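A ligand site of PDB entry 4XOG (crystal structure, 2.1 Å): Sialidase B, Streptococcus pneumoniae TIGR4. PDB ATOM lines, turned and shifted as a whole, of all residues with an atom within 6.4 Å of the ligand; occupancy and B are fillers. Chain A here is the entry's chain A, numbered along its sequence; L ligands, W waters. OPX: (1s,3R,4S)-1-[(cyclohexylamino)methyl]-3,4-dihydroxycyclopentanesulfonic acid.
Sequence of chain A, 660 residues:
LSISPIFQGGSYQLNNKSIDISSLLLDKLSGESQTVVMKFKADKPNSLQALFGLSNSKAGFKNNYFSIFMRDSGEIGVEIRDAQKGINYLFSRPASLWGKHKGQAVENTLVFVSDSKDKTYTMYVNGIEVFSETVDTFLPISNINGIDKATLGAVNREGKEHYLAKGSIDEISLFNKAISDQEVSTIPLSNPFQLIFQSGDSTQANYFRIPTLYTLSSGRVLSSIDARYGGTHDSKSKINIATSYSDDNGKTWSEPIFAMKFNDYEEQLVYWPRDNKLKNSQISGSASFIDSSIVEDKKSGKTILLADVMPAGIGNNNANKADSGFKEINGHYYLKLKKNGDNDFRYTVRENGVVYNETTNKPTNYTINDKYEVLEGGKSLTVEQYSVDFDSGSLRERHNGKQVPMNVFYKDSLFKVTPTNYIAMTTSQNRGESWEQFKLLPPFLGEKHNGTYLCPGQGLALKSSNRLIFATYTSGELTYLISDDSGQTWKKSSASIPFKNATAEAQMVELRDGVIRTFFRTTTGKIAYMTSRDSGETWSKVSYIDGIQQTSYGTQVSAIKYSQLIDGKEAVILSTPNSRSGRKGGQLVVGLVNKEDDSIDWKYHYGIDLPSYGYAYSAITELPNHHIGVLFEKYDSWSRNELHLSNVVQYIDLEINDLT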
ATOM      1  N   LEU A 213       2.962 -35.001  12.268  1.00  0.00           N
ATOM      2  CA  LEU A 213       4.222 -34.469  12.805  1.00  0.00           C
ATOM      3  C   LEU A 213       3.982 -33.045  13.239  1.00  0.00           C
ATOM      4  O   LEU A 213       3.261 -32.308  12.579  1.00  0.00           O
ATOM      5  CB  LEU A 213       5.346 -34.461  11.752  1.00  0.00           C
ATOM      6  CG  LEU A 213       5.972 -35.805  11.355  1.00  0.00           C
ATOM      7  CD1 LEU A 213       6.904 -35.640  10.142  1.00  0.00           C
ATOM      8  CD2 LEU A 213       6.751 -36.412  12.525  1.00  0.00           C
ATOM      9  N   TYR A 214       4.609 -32.646  14.337  1.00  0.00           N
ATOM     10  CA  TYR A 214       4.469 -31.296  14.830  1.00  0.00           C
ATOM     11  C   TYR A 214       5.734 -30.921  15.581  1.00  0.00           C
ATOM     12  O   TYR A 214       6.267 -31.727  16.377  1.00  0.00           O
ATOM     13  CB  TYR A 214       3.240 -31.204  15.753  1.00  0.00           C
ATOM     14  CG  TYR A 214       2.776 -29.773  16.031  1.00  0.00           C
ATOM     15  CD1 TYR A 214       3.412 -29.002  16.985  1.00  0.00           C
ATOM     16  CD2 TYR A 214       1.713 -29.217  15.327  1.00  0.00           C
ATOM     17  CE1 TYR A 214       3.004 -27.702  17.260  1.00  0.00           C
ATOM     18  CE2 TYR A 214       1.281 -27.906  15.591  1.00  0.00           C
ATOM     19  CZ  TYR A 214       1.929 -27.166  16.563  1.00  0.00           C
ATOM     20  OH  TYR A 214       1.538 -25.879  16.844  1.00  0.00           O
ATOM     21  N   THR A 215       6.250 -29.724  15.324  1.00  0.00           N
ATOM     22  CA  THR A 215       7.487 -29.275  15.974  1.00  0.00           C
ATOM     23  C   THR A 215       7.135 -28.401  17.161  1.00  0.00           C
ATOM     24  O   THR A 215       6.512 -27.344  17.007  1.00  0.00           O
ATOM     25  CB  THR A 215       8.384 -28.516  14.969  1.00  0.00           C
ATOM     26  OG1 THR A 215       8.657 -29.363  13.848  1.00  0.00           O
ATOM     27  CG2 THR A 215       9.706 -28.097  15.624  1.00  0.00           C
ATOM     28  N   LEU A 216       7.536 -28.853  18.344  1.00  0.00           N
ATOM     29  CA  LEU A 216       7.200 -28.173  19.586  1.00  0.00           C
ATOM     30  C   LEU A 216       8.233 -27.093  19.943  1.00  0.00           C
ATOM     31  O   LEU A 216       9.365 -27.134  19.471  1.00  0.00           O
ATOM     32  CB  LEU A 216       7.136 -29.199  20.723  1.00  0.00           C
ATOM     33  CG  LEU A 216       6.185 -30.376  20.546  1.00  0.00           C
ATOM     34  CD1 LEU A 216       6.268 -31.276  21.801  1.00  0.00           C
ATOM     35  CD2 LEU A 216       4.753 -29.891  20.330  1.00  0.00           C
ATOM     36  N   GLU A 296       0.271 -27.247  19.576  1.00  0.00           N
ATOM     37  CA  GLU A 296       0.859 -26.817  20.850  1.00  0.00           C
ATOM     38  C   GLU A 296       0.276 -25.460  21.271  1.00  0.00           C
ATOM     39  O   GLU A 296       0.089 -24.557  20.439  1.00  0.00           O
ATOM     40  CB  GLU A 296       2.403 -26.737  20.776  1.00  0.00           C
ATOM     41  CG  GLU A 296       3.060 -26.243  22.066  1.00  0.00           C
ATOM     42  CD  GLU A 296       4.565 -26.452  22.078  1.00  0.00           C
ATOM     43  OE1 GLU A 296       5.264 -25.853  21.236  1.00  0.00           O
ATOM     44  OE2 GLU A 296       5.041 -27.240  22.937  1.00  0.00           O
ATOM     45  N   LYS A 298       0.691 -22.039  23.239  1.00  0.00           N
ATOM     46  CA  LYS A 298       1.732 -21.143  23.745  1.00  0.00           C
ATOM     47  C   LYS A 298       1.434 -20.717  25.174  1.00  0.00           C
ATOM     48  O   LYS A 298       2.341 -20.640  26.021  1.00  0.00           O
ATOM     49  CB  LYS A 298       1.884 -19.908  22.835  1.00  0.00           C
ATOM     50  CG  LYS A 298       2.578 -20.182  21.487  1.00  0.00           C
ATOM     51  CD  LYS A 298       2.081 -19.262  20.336  1.00  0.00           C
ATOM     52  CE  LYS A 298       2.075 -19.972  18.941  1.00  0.00           C
ATOM     53  NZ  LYS A 298       3.337 -19.864  18.106  1.00  0.00           N
ATOM     54  N   GLN A 458      -1.969 -31.499  11.593  1.00  0.00           N
ATOM     55  CA  GLN A 458      -1.674 -30.494  12.601  1.00  0.00           C
ATOM     56  C   GLN A 458      -2.881 -29.581  12.798  1.00  0.00           C
ATOM     57  O   GLN A 458      -3.619 -29.297  11.847  1.00  0.00           O
ATOM     58  CB  GLN A 458      -0.484 -29.643  12.147  1.00  0.00           C
ATOM     59  CG  GLN A 458       0.750 -30.412  11.711  1.00  0.00           C
ATOM     60  CD  GLN A 458       1.887 -29.482  11.329  1.00  0.00           C
ATOM     61  OE1 GLN A 458       1.671 -28.274  11.078  1.00  0.00           O
ATOM     62  NE2 GLN A 458       3.090 -30.021  11.259  1.00  0.00           N
ATOM     63  N   GLY A 459      -3.075 -29.132  14.033  1.00  0.00           N
ATOM     64  CA  GLY A 459      -3.938 -27.989  14.275  1.00  0.00           C
ATOM     65  C   GLY A 459      -3.059 -26.772  14.047  1.00  0.00           C
ATOM     66  O   GLY A 459      -1.859 -26.922  13.807  1.00  0.00           O
ATOM     67  N   LEU A 460      -3.643 -25.573  14.130  1.00  0.00           N
ATOM     68  CA  LEU A 460      -2.884 -24.348  13.914  1.00  0.00           C
ATOM     69  C   LEU A 460      -2.888 -23.491  15.166  1.00  0.00           C
ATOM     70  O   LEU A 460      -3.941 -23.175  15.718  1.00  0.00           O
ATOM     71  CB  LEU A 460      -3.482 -23.548  12.748  1.00  0.00           C
ATOM     72  CG  LEU A 460      -2.843 -22.178  12.456  1.00  0.00           C
ATOM     73  CD1 LEU A 460      -1.441 -22.361  11.875  1.00  0.00           C
ATOM     74  CD2 LEU A 460      -3.699 -21.367  11.499  1.00  0.00           C
ATOM     75  N   ALA A 461      -1.693 -23.132  15.618  1.00  0.00           N
ATOM     76  CA  ALA A 461      -1.503 -22.150  16.686  1.00  0.00           C
ATOM     77  C   ALA A 461      -1.095 -20.829  16.030  1.00  0.00           C
ATOM     78  O   ALA A 461      -0.067 -20.751  15.373  1.00  0.00           O
ATOM     79  CB  ALA A 461      -0.406 -22.606  17.681  1.00  0.00           C
ATOM     80  N   LYS A 463       0.399 -17.114  15.474  1.00  0.00           N
ATOM     81  CA  LYS A 463       1.667 -16.572  15.968  1.00  0.00           C
ATOM     82  C   LYS A 463       1.480 -15.375  16.908  1.00  0.00           C
ATOM     83  O   LYS A 463       2.247 -15.193  17.857  1.00  0.00           O
ATOM     84  CB  LYS A 463       2.561 -16.140  14.788  1.00  0.00           C
ATOM     85  CG  LYS A 463       2.936 -17.267  13.819  1.00  0.00           C
ATOM     86  CD  LYS A 463       4.334 -17.838  14.099  1.00  0.00           C
ATOM     87  CE  LYS A 463       4.900 -18.553  12.855  1.00  0.00           C
ATOM     88  NZ  LYS A 463       3.884 -19.442  12.197  1.00  0.00           N
ATOM     89  N   ALA A 559       0.658 -29.528   4.856  1.00  0.00           N
ATOM     90  CA  ALA A 559       1.105 -28.196   4.461  1.00  0.00           C
ATOM     91  C   ALA A 559       1.714 -27.425   5.623  1.00  0.00           C
ATOM     92  O   ALA A 559       1.138 -27.385   6.717  1.00  0.00           O
ATOM     93  CB  ALA A 559      -0.060 -27.407   3.874  1.00  0.00           C
ATOM     94  N   ILE A 560       2.856 -26.797   5.364  1.00  0.00           N
ATOM     95  CA  ILE A 560       3.494 -25.958   6.355  1.00  0.00           C
ATOM     96  C   ILE A 560       3.947 -24.649   5.738  1.00  0.00           C
ATOM     97  O   ILE A 560       4.126 -24.533   4.524  1.00  0.00           O
ATOM     98  CB  ILE A 560       4.737 -26.655   6.966  1.00  0.00           C
ATOM     99  CG1 ILE A 560       5.696 -27.059   5.858  1.00  0.00           C
ATOM    100  CG2 ILE A 560       4.318 -27.870   7.803  1.00  0.00           C
ATOM    101  CD1 ILE A 560       7.046 -27.551   6.373  1.00  0.00           C
ATOM    102  N   LYS A 561       4.152 -23.651   6.598  1.00  0.00           N
ATOM    103  CA  LYS A 561       4.803 -22.418   6.215  1.00  0.00           C
ATOM    104  C   LYS A 561       6.257 -22.534   6.655  1.00  0.00           C
ATOM    105  O   LYS A 561       6.535 -22.733   7.844  1.00  0.00           O
ATOM    106  CB  LYS A 561       4.110 -21.251   6.940  1.00  0.00           C
ATOM    107  CG  LYS A 561       4.858 -19.932   6.899  1.00  0.00           C
ATOM    108  CD  LYS A 561       4.404 -19.112   5.712  1.00  0.00           C
ATOM    109  CE  LYS A 561       5.085 -17.745   5.729  1.00  0.00           C
ATOM    110  NZ  LYS A 561       6.534 -17.890   5.429  1.00  0.00           N
ATOM    111  N   SER A 563       9.970 -21.451   7.787  1.00  0.00           N
ATOM    112  CA  SER A 563      10.373 -20.293   8.605  1.00  0.00           C
ATOM    113  C   SER A 563      11.387 -19.407   7.884  1.00  0.00           C
ATOM    114  O   SER A 563      11.590 -18.248   8.267  1.00  0.00           O
ATOM    115  CB  SER A 563      10.963 -20.737   9.941  1.00  0.00           C
ATOM    116  OG  SER A 563      12.298 -21.196   9.740  1.00  0.00           O
ATOM    117  N   ILE A 620       4.254 -33.422   7.287  1.00  0.00           N
ATOM    118  CA  ILE A 620       5.523 -32.716   7.147  1.00  0.00           C
ATOM    119  C   ILE A 620       5.696 -31.702   8.259  1.00  0.00           C
ATOM    120  O   ILE A 620       4.727 -31.103   8.727  1.00  0.00           O
ATOM    121  CB  ILE A 620       5.683 -32.021   5.783  1.00  0.00           C
ATOM    122  CG1 ILE A 620       4.513 -31.077   5.515  1.00  0.00           C
ATOM    123  CG2 ILE A 620       5.797 -33.070   4.656  1.00  0.00           C
ATOM    124  CD1 ILE A 620       4.629 -30.401   4.176  1.00  0.00           C
ATOM    125  N   THR A 621       6.940 -31.521   8.679  1.00  0.00           N
ATOM    126  CA  THR A 621       7.210 -30.481   9.648  1.00  0.00           C
ATOM    127  C   THR A 621       8.624 -29.975   9.452  1.00  0.00           C
ATOM    128  O   THR A 621       9.520 -30.744   9.070  1.00  0.00           O
ATOM    129  CB  THR A 621       6.928 -30.953  11.109  1.00  0.00           C
ATOM    130  OG1 THR A 621       6.776 -29.809  11.966  1.00  0.00           O
ATOM    131  CG2 THR A 621       8.050 -31.856  11.632  1.00  0.00           C
ATOM    132  N   GLU A 622       8.798 -28.679   9.686  1.00  0.00           N
ATOM    133  CA  GLU A 622      10.113 -28.079   9.722  1.00  0.00           C
ATOM    134  C   GLU A 622      10.745 -28.485  11.041  1.00  0.00           C
ATOM    135  O   GLU A 622      10.233 -28.146  12.125  1.00  0.00           O
ATOM    136  CB  GLU A 622      10.041 -26.549   9.611  1.00  0.00           C
ATOM    137  CG  GLU A 622      11.422 -25.884   9.515  1.00  0.00           C
ATOM    138  CD  GLU A 622      11.340 -24.394   9.254  1.00  0.00           C
ATOM    139  OE1 GLU A 622      10.217 -23.891   8.974  1.00  0.00           O
ATOM    140  OE2 GLU A 622      12.398 -23.709   9.354  1.00  0.00           O
ATOM    141  N   LEU A 623      11.848 -29.227  10.967  1.00  0.00           N
ATOM    142  CA  LEU A 623      12.603 -29.604  12.162  1.00  0.00           C
ATOM    143  C   LEU A 623      13.292 -28.350  12.686  1.00  0.00           C
ATOM    144  O   LEU A 623      13.443 -27.378  11.944  1.00  0.00           O
ATOM    145  CB  LEU A 623      13.614 -30.692  11.786  1.00  0.00           C
ATOM    146  CG  LEU A 623      12.936 -31.901  11.106  1.00  0.00           C
ATOM    147  CD1 LEU A 623      13.943 -32.863  10.487  1.00  0.00           C
ATOM    148  CD2 LEU A 623      12.040 -32.635  12.098  1.00  0.00           C
ATOM    149  N   PRO A 624      13.697 -28.351  13.976  1.00  0.00           N
ATOM    150  CA  PRO A 624      14.367 -27.171  14.542  1.00  0.00           C
ATOM    151  C   PRO A 624      15.625 -26.709  13.798  1.00  0.00           C
ATOM    152  O   PRO A 624      15.959 -25.514  13.877  1.00  0.00           O
ATOM    153  CB  PRO A 624      14.754 -27.640  15.946  1.00  0.00           C
ATOM    154  CG  PRO A 624      13.648 -28.597  16.311  1.00  0.00           C
ATOM    155  CD  PRO A 624      13.330 -29.330  15.015  1.00  0.00           C
ATOM    156  N   ASN A 625      16.321 -27.620  13.117  1.00  0.00           N
ATOM    157  CA  ASN A 625      17.528 -27.249  12.382  1.00  0.00           C
ATOM    158  C   ASN A 625      17.223 -26.834  10.954  1.00  0.00           C
ATOM    159  O   ASN A 625      18.124 -26.747  10.132  1.00  0.00           O
ATOM    160  CB  ASN A 625      18.529 -28.412  12.374  1.00  0.00           C
ATOM    161  CG  ASN A 625      17.972 -29.654  11.696  1.00  0.00           C
ATOM    162  OD1 ASN A 625      16.819 -29.647  11.252  1.00  0.00           O
ATOM    163  ND2 ASN A 625      18.774 -30.707  11.605  1.00  0.00           N
ATOM    164  N   HIS A 626      15.933 -26.630  10.651  1.00  0.00           N
ATOM    165  CA  HIS A 626      15.456 -26.165   9.340  1.00  0.00           C
ATOM    166  C   HIS A 626      15.466 -27.219   8.216  1.00  0.00           C
ATOM    167  O   HIS A 626      15.250 -26.890   7.047  1.00  0.00           O
ATOM    168  CB  HIS A 626      16.174 -24.886   8.896  1.00  0.00           C
ATOM    169  CG  HIS A 626      16.088 -23.775   9.916  1.00  0.00           C
ATOM    170  ND1 HIS A 626      14.884 -23.333  10.401  1.00  0.00           N
ATOM    171  CD2 HIS A 626      17.054 -23.053  10.530  1.00  0.00           C
ATOM    172  CE1 HIS A 626      15.115 -22.345  11.287  1.00  0.00           C
ATOM    173  NE2 HIS A 626      16.419 -22.180  11.381  1.00  0.00           N
HETATM  174  CAF OPX L   1      11.818 -23.905  13.234  1.00  0.00           C
HETATM  175  CAG OPX L   1      11.277 -22.708  14.001  1.00  0.00           C
HETATM  176  CAH OPX L   1      10.993 -25.146  13.448  1.00  0.00           C
HETATM  177  CAI OPX L   1       9.786 -22.506  13.781  1.00  0.00           C
HETATM  178  CAJ OPX L   1       9.499 -24.917  13.293  1.00  0.00           C
HETATM  179  CAK OPX L   1       6.750 -24.658  14.318  1.00  0.00           C
HETATM  180  CAL OPX L   1       4.998 -24.926  12.501  1.00  0.00           C
HETATM  181  CAM OPX L   1       4.513 -25.765  14.679  1.00  0.00           C
HETATM  182  CAO OPX L   1       3.936 -25.980  12.432  1.00  0.00           C
HETATM  183  CAP OPX L   1       4.136 -26.754  13.609  1.00  0.00           C
HETATM  184  CAQ OPX L   1       9.001 -23.757  14.112  1.00  0.00           C
HETATM  185  CAR OPX L   1       5.231 -24.671  13.951  1.00  0.00           C
HETATM  186  NAN OPX L   1       7.565 -23.540  13.845  1.00  0.00           N
HETATM  187  OAA OPX L   1       4.451 -22.856  15.744  1.00  0.00           O
HETATM  188  OAB OPX L   1       3.028 -23.171  13.815  1.00  0.00           O
HETATM  189  OAC OPX L   1       4.164 -26.744  11.268  1.00  0.00           O
HETATM  190  OAD OPX L   1       5.228 -27.611  13.439  1.00  0.00           O
HETATM  191  OAE OPX L   1       5.157 -22.067  13.535  1.00  0.00           O
HETATM  192  SAS OPX L   1       4.420 -23.116  14.288  1.00  0.00           S
HETATM  193  O   HOH W   1       4.745 -21.836  10.598  1.00  0.00           O
HETATM  194  O   HOH W   2       7.169 -22.540  11.351  1.00  0.00           O
HETATM  195  O   HOH W   3       3.353 -24.112  17.746  1.00  0.00           O
HETATM  196  O   HOH W   4       7.002 -21.590  15.863  1.00  0.00           O
HETATM  197  O   HOH W   5       0.691 -24.540  14.689  1.00  0.00           O
HETATM  198  O   HOH W   6       3.382 -24.346   9.278  1.00  0.00           O
HETATM  199  O   HOH W   7       6.755 -26.818  10.001  1.00  0.00           O
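OE1 of Gln 458 is in hydrogen-bond range of OAC of the ligand (2.9 Å). OAD of the ligand sits at hydrogen-bond distance from OG1 of Thr 621 (3.1 Å). NZ of Lys 463 lies within salt-bridge range of OAE of the ligand (3.2 Å). The side-chain amino group of Lys 298 is in salt-bridge range of an oxygen (OAA) of the ligand (3.97 Å). N of Thr 215 is in hydrogen-bond range of OAD of the ligand.
The side-chain hydroxyl (OG1) of Thr 215 lies within hydrogen-bond range of the backbone carbonyl oxygen (O) of Glu 622 (2.6 Å). The side-chain carboxylate (OE2) of Glu 622 lies within hydrogen-bond range of the side-chain hydroxyl (OG) of Ser 563 (2.5 Å). The side-chain hydroxyl of Thr 215 sits at hydrogen-bond distance from the side-chain hydroxyl of Thr 621, 2.7 Å away. The side-chain amide nitrogen of Gln 458 is in hydrogen-bond range of the backbone carbonyl oxygen of Leu 213, at 2.6 Å. A ring nitrogen (ND1) of His 626 is in hydrogen-bond range of the side-chain carboxylate of Glu 622 (2.7 Å). The backbone carbonyl oxygen (O) of Ile 620 is in hydrogen-bond range of the side-chain amide nitrogen (NE2) of Gln 458, at 3.2 Å. The side-chain hydroxyl (OH) of Tyr 214 sits at hydrogen-bond distance from the backbone NH (N) of Glu 296, at 3.3 Å.
Tyr 214 touches the ligand (CZ to CAM, 3.5 Å). CG2 of Ile 560 touches OAC of the ligand (3.6 Å). Glu 622 touches the ligand. Leu 623 touches the ligand (O to CAH, 3.6 Å). Hydrophobic or aromatic side chains that line the ligand: Tyr 214 and Ile 560. Within 4 Å of the ligand: Tyr 214, Thr 215, Lys 298, Gln 458, Lys 463, Ile 560, Thr 621, Glu 622 and Leu 623. Along chain A the residues within 4 Å of the ligand span positions 214 to 623.
Water W3 bridges an oxygen (OAA) of the ligand (2.6 Å) and the side-chain hydroxyl of Tyr 214 (2.7 Å). Water W5 lies within hydrogen-bond range of OH of Tyr 214, OAB of the ligand and N of Ala 461. Water W7 lies within hydrogen-bond range of the backbone NH of Glu 622 (2.8 Å) and an oxygen (OAC) of the ligand (2.9 Å). Water W1 lies within hydrogen-bond range of an oxygen (OAE) of the ligand (3.0 Å), the side-chain amino group of Lys 463 (3.0 Å) and the backbone carbonyl oxygen of Lys 561 (3.4 Å). Water W6 bridges the backbone NH of Lys 561 (2.9 Å) and an oxygen (OAC) of the ligand (3.2 Å).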
